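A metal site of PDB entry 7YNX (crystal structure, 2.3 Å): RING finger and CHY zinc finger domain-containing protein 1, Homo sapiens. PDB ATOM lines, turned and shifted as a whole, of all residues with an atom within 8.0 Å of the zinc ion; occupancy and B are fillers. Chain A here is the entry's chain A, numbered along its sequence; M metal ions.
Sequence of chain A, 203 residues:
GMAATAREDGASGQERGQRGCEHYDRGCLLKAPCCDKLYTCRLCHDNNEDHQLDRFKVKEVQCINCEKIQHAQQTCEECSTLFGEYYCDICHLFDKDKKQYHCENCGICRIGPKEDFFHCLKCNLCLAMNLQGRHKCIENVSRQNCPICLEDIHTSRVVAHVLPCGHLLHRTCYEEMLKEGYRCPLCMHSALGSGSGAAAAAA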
ATOM      1  N   ARG A  55     -25.523   0.636  -0.344  1.00  0.00           N
ATOM      2  CA  ARG A  55     -26.388   0.354   0.792  1.00  0.00           C
ATOM      3  C   ARG A  55     -26.455   1.524   1.761  1.00  0.00           C
ATOM      4  O   ARG A  55     -27.499   1.756   2.389  1.00  0.00           O
ATOM      5  CB  ARG A  55     -25.922  -0.906   1.503  1.00  0.00           C
ATOM      6  CG  ARG A  55     -24.543  -0.763   2.104  1.00  0.00           C
ATOM      7  CD  ARG A  55     -23.918  -2.117   2.344  1.00  0.00           C
ATOM      8  NE  ARG A  55     -24.695  -2.909   3.299  1.00  0.00           N
ATOM      9  CZ  ARG A  55     -24.219  -3.974   3.933  1.00  0.00           C
ATOM     10  NH1 ARG A  55     -22.970  -4.385   3.698  1.00  0.00           N
ATOM     11  NH2 ARG A  55     -24.989  -4.649   4.771  1.00  0.00           N
ATOM     12  N   PHE A  56     -25.366   2.294   1.894  1.00  0.00           N
ATOM     13  CA  PHE A  56     -25.388   3.453   2.762  1.00  0.00           C
ATOM     14  C   PHE A  56     -26.218   4.601   2.171  1.00  0.00           C
ATOM     15  O   PHE A  56     -26.602   5.511   2.906  1.00  0.00           O
ATOM     16  CB  PHE A  56     -23.970   3.954   3.054  1.00  0.00           C
ATOM     17  CG  PHE A  56     -22.984   2.853   3.348  1.00  0.00           C
ATOM     18  CD1 PHE A  56     -23.071   2.114   4.520  1.00  0.00           C
ATOM     19  CD2 PHE A  56     -21.955   2.572   2.454  1.00  0.00           C
ATOM     20  CE1 PHE A  56     -22.151   1.117   4.795  1.00  0.00           C
ATOM     21  CE2 PHE A  56     -21.040   1.570   2.723  1.00  0.00           C
ATOM     22  CZ  PHE A  56     -21.140   0.849   3.891  1.00  0.00           C
ATOM     23  N   TYR A  86     -32.419  -7.709  13.991  1.00  0.00           N
ATOM     24  CA  TYR A  86     -31.260  -6.832  13.982  1.00  0.00           C
ATOM     25  C   TYR A  86     -31.465  -5.765  12.921  1.00  0.00           C
ATOM     26  O   TYR A  86     -31.836  -6.075  11.774  1.00  0.00           O
ATOM     27  CB  TYR A  86     -29.967  -7.628  13.710  1.00  0.00           C
ATOM     28  CG  TYR A  86     -28.745  -6.747  13.633  1.00  0.00           C
ATOM     29  CD1 TYR A  86     -28.135  -6.273  14.778  1.00  0.00           C
ATOM     30  CD2 TYR A  86     -28.212  -6.361  12.401  1.00  0.00           C
ATOM     31  CE1 TYR A  86     -27.029  -5.457  14.724  1.00  0.00           C
ATOM     32  CE2 TYR A  86     -27.091  -5.539  12.331  1.00  0.00           C
ATOM     33  CZ  TYR A  86     -26.498  -5.096  13.499  1.00  0.00           C
ATOM     34  OH  TYR A  86     -25.408  -4.286  13.447  1.00  0.00           O
ATOM     35  N   TYR A  87     -31.232  -4.519  13.291  1.00  0.00           N
ATOM     36  CA  TYR A  87     -31.329  -3.424  12.350  1.00  0.00           C
ATOM     37  C   TYR A  87     -30.170  -2.473  12.568  1.00  0.00           C
ATOM     38  O   TYR A  87     -29.956  -2.029  13.699  1.00  0.00           O
ATOM     39  CB  TYR A  87     -32.644  -2.672  12.494  1.00  0.00           C
ATOM     40  CG  TYR A  87     -32.640  -1.348  11.801  1.00  0.00           C
ATOM     41  CD1 TYR A  87     -32.356  -1.246  10.451  1.00  0.00           C
ATOM     42  CD2 TYR A  87     -32.915  -0.181  12.496  1.00  0.00           C
ATOM     43  CE1 TYR A  87     -32.335  -0.035   9.806  1.00  0.00           C
ATOM     44  CE2 TYR A  87     -32.910   1.059  11.855  1.00  0.00           C
ATOM     45  CZ  TYR A  87     -32.628   1.121  10.511  1.00  0.00           C
ATOM     46  OH  TYR A  87     -32.625   2.327   9.854  1.00  0.00           O
ATOM     47  N   CYS A  88     -29.440  -2.171  11.492  1.00  0.00           N
ATOM     48  CA  CYS A  88     -28.343  -1.215  11.512  1.00  0.00           C
ATOM     49  C   CYS A  88     -28.682  -0.074  10.572  1.00  0.00           C
ATOM     50  O   CYS A  88     -28.833  -0.300   9.364  1.00  0.00           O
ATOM     51  CB  CYS A  88     -27.023  -1.841  11.095  1.00  0.00           C
ATOM     52  SG  CYS A  88     -25.778  -0.582  10.691  1.00  0.00           S
ATOM     53  N   ASP A  89     -28.792   1.143  11.113  1.00  0.00           N
ATOM     54  CA  ASP A  89     -29.196   2.303  10.329  1.00  0.00           C
ATOM     55  C   ASP A  89     -28.086   2.899   9.486  1.00  0.00           C
ATOM     56  O   ASP A  89     -28.323   3.899   8.793  1.00  0.00           O
ATOM     57  CB  ASP A  89     -29.780   3.388  11.244  1.00  0.00           C
ATOM     58  CG  ASP A  89     -28.921   3.626  12.477  1.00  0.00           C
ATOM     59  OD1 ASP A  89     -27.979   2.845  12.726  1.00  0.00           O
ATOM     60  OD2 ASP A  89     -29.207   4.606  13.214  1.00  0.00           O
ATOM     61  N   ILE A  90     -26.878   2.334   9.515  1.00  0.00           N
ATOM     62  CA  ILE A  90     -25.797   2.775   8.639  1.00  0.00           C
ATOM     63  C   ILE A  90     -25.766   1.972   7.338  1.00  0.00           C
ATOM     64  O   ILE A  90     -25.825   2.532   6.245  1.00  0.00           O
ATOM     65  CB  ILE A  90     -24.451   2.708   9.377  1.00  0.00           C
ATOM     66  CG1 ILE A  90     -24.510   3.571  10.637  1.00  0.00           C
ATOM     67  CG2 ILE A  90     -23.326   3.141   8.443  1.00  0.00           C
ATOM     68  CD1 ILE A  90     -23.252   3.502  11.490  1.00  0.00           C
ATOM     69  N   CYS A  91     -25.671   0.641   7.461  1.00  0.00           N
ATOM     70  CA  CYS A  91     -25.763  -0.217   6.285  1.00  0.00           C
ATOM     71  C   CYS A  91     -27.186  -0.383   5.783  1.00  0.00           C
ATOM     72  O   CYS A  91     -27.368  -0.891   4.665  1.00  0.00           O
ATOM     73  CB  CYS A  91     -25.193  -1.598   6.590  1.00  0.00           C
ATOM     74  SG  CYS A  91     -23.515  -1.600   7.212  1.00  0.00           S
ATOM     75  N   HIS A  92     -28.189  -0.022   6.592  1.00  0.00           N
ATOM     76  CA  HIS A  92     -29.593  -0.302   6.274  1.00  0.00           C
ATOM     77  C   HIS A  92     -29.840  -1.795   6.072  1.00  0.00           C
ATOM     78  O   HIS A  92     -30.529  -2.217   5.144  1.00  0.00           O
ATOM     79  CB  HIS A  92     -30.058   0.524   5.071  1.00  0.00           C
ATOM     80  CG  HIS A  92     -29.760   1.978   5.234  1.00  0.00           C
ATOM     81  ND1 HIS A  92     -28.724   2.610   4.571  1.00  0.00           N
ATOM     82  CD2 HIS A  92     -30.312   2.907   6.056  1.00  0.00           C
ATOM     83  CE1 HIS A  92     -28.676   3.872   4.951  1.00  0.00           C
ATOM     84  NE2 HIS A  92     -29.633   4.077   5.850  1.00  0.00           N
ATOM     85  N   LEU A  93     -29.271  -2.608   6.956  1.00  0.00           N
ATOM     86  CA  LEU A  93     -29.415  -4.058   6.926  1.00  0.00           C
ATOM     87  C   LEU A  93     -30.499  -4.483   7.911  1.00  0.00           C
ATOM     88  O   LEU A  93     -30.570  -3.963   9.023  1.00  0.00           O
ATOM     89  CB  LEU A  93     -28.088  -4.739   7.259  1.00  0.00           C
ATOM     90  CG  LEU A  93     -28.040  -6.265   7.156  1.00  0.00           C
ATOM     91  CD1 LEU A  93     -26.717  -6.755   6.595  1.00  0.00           C
ATOM     92  CD2 LEU A  93     -28.284  -6.894   8.511  1.00  0.00           C
ATOM     93  N   GLN A 100     -25.036 -10.081  14.875  1.00  0.00           N
ATOM     94  CA  GLN A 100     -24.344  -9.074  14.098  1.00  0.00           C
ATOM     95  C   GLN A 100     -23.905  -7.897  14.968  1.00  0.00           C
ATOM     96  O   GLN A 100     -24.491  -7.595  16.011  1.00  0.00           O
ATOM     97  CB  GLN A 100     -25.246  -8.526  12.982  1.00  0.00           C
ATOM     98  CG  GLN A 100     -25.860  -9.575  12.085  1.00  0.00           C
ATOM     99  CD  GLN A 100     -27.234 -10.000  12.573  1.00  0.00           C
ATOM    100  OE1 GLN A 100     -27.526  -9.961  13.766  1.00  0.00           O
ATOM    101  NE2 GLN A 100     -28.081 -10.435  11.642  1.00  0.00           N
ATOM    102  N   TYR A 101     -22.853  -7.232  14.505  1.00  0.00           N
ATOM    103  CA  TYR A 101     -22.439  -5.940  14.997  1.00  0.00           C
ATOM    104  C   TYR A 101     -21.932  -5.147  13.815  1.00  0.00           C
ATOM    105  O   TYR A 101     -21.451  -5.701  12.818  1.00  0.00           O
ATOM    106  CB  TYR A 101     -21.343  -6.057  16.062  1.00  0.00           C
ATOM    107  CG  TYR A 101     -20.039  -6.601  15.530  1.00  0.00           C
ATOM    108  CD1 TYR A 101     -19.895  -7.945  15.278  1.00  0.00           C
ATOM    109  CD2 TYR A 101     -18.967  -5.766  15.246  1.00  0.00           C
ATOM    110  CE1 TYR A 101     -18.714  -8.461  14.776  1.00  0.00           C
ATOM    111  CE2 TYR A 101     -17.775  -6.265  14.736  1.00  0.00           C
ATOM    112  CZ  TYR A 101     -17.656  -7.616  14.509  1.00  0.00           C
ATOM    113  OH  TYR A 101     -16.478  -8.156  14.013  1.00  0.00           O
ATOM    114  N   HIS A 102     -22.064  -3.829  13.913  1.00  0.00           N
ATOM    115  CA  HIS A 102     -21.526  -2.936  12.897  1.00  0.00           C
ATOM    116  C   HIS A 102     -20.169  -2.433  13.371  1.00  0.00           C
ATOM    117  O   HIS A 102     -20.059  -1.902  14.482  1.00  0.00           O
ATOM    118  CB  HIS A 102     -22.468  -1.761  12.628  1.00  0.00           C
ATOM    119  CG  HIS A 102     -21.908  -0.750  11.679  1.00  0.00           C
ATOM    120  ND1 HIS A 102     -22.029  -0.868  10.314  1.00  0.00           N
ATOM    121  CD2 HIS A 102     -21.177   0.367  11.900  1.00  0.00           C
ATOM    122  CE1 HIS A 102     -21.426   0.152   9.717  1.00  0.00           C
ATOM    123  NE2 HIS A 102     -20.903   0.914  10.664  1.00  0.00           N
ATOM    124  N   CYS A 103     -19.161  -2.602  12.537  1.00  0.00           N
ATOM    125  CA  CYS A 103     -17.789  -2.205  12.845  1.00  0.00           C
ATOM    126  C   CYS A 103     -17.446  -0.960  12.026  1.00  0.00           C
ATOM    127  O   CYS A 103     -17.503  -0.993  10.798  1.00  0.00           O
ATOM    128  CB  CYS A 103     -16.815  -3.342  12.544  1.00  0.00           C
ATOM    129  SG  CYS A 103     -15.117  -2.789  12.468  1.00  0.00           S
ATOM    130  N   GLU A 104     -17.073   0.123  12.722  1.00  0.00           N
ATOM    131  CA  GLU A 104     -16.831   1.385  12.014  1.00  0.00           C
ATOM    132  C   GLU A 104     -15.623   1.315  11.094  1.00  0.00           C
ATOM    133  O   GLU A 104     -15.603   1.988  10.059  1.00  0.00           O
ATOM    134  CB  GLU A 104     -16.637   2.531  13.009  1.00  0.00           C
ATOM    135  CG  GLU A 104     -17.835   2.809  13.932  1.00  0.00           C
ATOM    136  CD  GLU A 104     -18.886   3.739  13.315  1.00  0.00           C
ATOM    137  OE1 GLU A 104     -20.093   3.406  13.400  1.00  0.00           O
ATOM    138  OE2 GLU A 104     -18.517   4.801  12.761  1.00  0.00           O
ATOM    139  N   GLY A 107     -16.489  -0.573   8.194  1.00  0.00           N
ATOM    140  CA  GLY A 107     -17.488   0.221   7.511  1.00  0.00           C
ATOM    141  C   GLY A 107     -18.761  -0.517   7.224  1.00  0.00           C
ATOM    142  O   GLY A 107     -19.661   0.066   6.591  1.00  0.00           O
ATOM    143  N   ILE A 108     -18.903  -1.769   7.664  1.00  0.00           N
ATOM    144  CA  ILE A 108     -20.068  -2.583   7.370  1.00  0.00           C
ATOM    145  C   ILE A 108     -20.443  -3.368   8.623  1.00  0.00           C
ATOM    146  O   ILE A 108     -19.753  -3.310   9.652  1.00  0.00           O
ATOM    147  CB  ILE A 108     -19.837  -3.543   6.191  1.00  0.00           C
ATOM    148  CG1 ILE A 108     -18.516  -4.313   6.375  1.00  0.00           C
ATOM    149  CG2 ILE A 108     -19.882  -2.800   4.847  1.00  0.00           C
ATOM    150  CD1 ILE A 108     -18.349  -5.508   5.438  1.00  0.00           C
ATOM    151  N   CYS A 109     -21.528  -4.122   8.519  1.00  0.00           N
ATOM    152  CA  CYS A 109     -21.901  -5.041   9.578  1.00  0.00           C
ATOM    153  C   CYS A 109     -21.174  -6.377   9.421  1.00  0.00           C
ATOM    154  O   CYS A 109     -21.043  -6.902   8.313  1.00  0.00           O
ATOM    155  CB  CYS A 109     -23.414  -5.270   9.577  1.00  0.00           C
ATOM    156  SG  CYS A 109     -24.316  -4.065  10.581  1.00  0.00           S
ATOM    157  N   ARG A 110     -20.693  -6.909  10.538  1.00  0.00           N
ATOM    158  CA  ARG A 110     -20.056  -8.205  10.586  1.00  0.00           C
ATOM    159  C   ARG A 110     -20.969  -9.230  11.263  1.00  0.00           C
ATOM    160  O   ARG A 110     -21.877  -8.877  12.018  1.00  0.00           O
ATOM    161  CB  ARG A 110     -18.723  -8.117  11.328  1.00  0.00           C
ATOM    162  CG  ARG A 110     -17.640  -7.353  10.564  1.00  0.00           C
ATOM    163  CD  ARG A 110     -17.220  -8.129   9.313  1.00  0.00           C
ATOM    164  NE  ARG A 110     -16.315  -7.350   8.479  1.00  0.00           N
ATOM    165  CZ  ARG A 110     -15.931  -7.712   7.266  1.00  0.00           C
ATOM    166  NH1 ARG A 110     -16.371  -8.857   6.750  1.00  0.00           N
ATOM    167  NH2 ARG A 110     -15.125  -6.924   6.578  1.00  0.00           N
ATOM    168  N   ALA A 203     -22.237  -9.408   7.279  1.00  0.00           N
ATOM    169  CA  ALA A 203     -23.623  -9.769   7.558  1.00  0.00           C
ATOM    170  C   ALA A 203     -24.514  -9.579   6.333  1.00  0.00           C
ATOM    171  O   ALA A 203     -25.523 -10.261   6.170  1.00  0.00           O
ATOM    172  CB  ALA A 203     -24.159  -8.942   8.737  1.00  0.00           C
ATOM    173  OXT ALA A 203     -24.231  -8.742   5.471  1.00  0.00           O
HETATM  174 ZN    ZN M   1     -23.825  -1.808   9.680  1.00  0.00          ZN
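ND1 of His 102 lies close to O of Ile 108, 3.4 Å away. The backbone NH (N) of His 102 is in hydrogen-bond range of the side-chain hydroxyl (OH) of Tyr 86, 3.4 Å away. SG of Cys 109 lies close to OH of Tyr 86 (3.1 Å). The backbone carbonyl oxygen (O) of Cys 109 lies within hydrogen-bond range of the backbone NH (N) of Ala 203 (3.0 Å). SG of Cys 88 sits close to N of Ile 90, 3.3 Å away. N of Cys 88 lies within hydrogen-bond range of O of Leu 93 (3.3 Å). The backbone carbonyl oxygen of Ile 108 sits at hydrogen-bond distance from the backbone NH of Cys 103.
ND1 of His 102 is bound to the zinc ion, 2.1 Å away. The zinc ion is bound by the side-chain sulfur (SG) of Cys 109 (2.5 Å). The zinc ion is bound by SG of Cys 91 (2.5 Å). The zinc ion is bound by the side-chain sulfur (SG) of Cys 88 (2.5 Å). The zinc ion has four donor atoms within binding distance.
Merely in contact with the zinc ion: Ile 108. Of the 20 residues printed, 5 come within 4 Å of the zinc ion.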
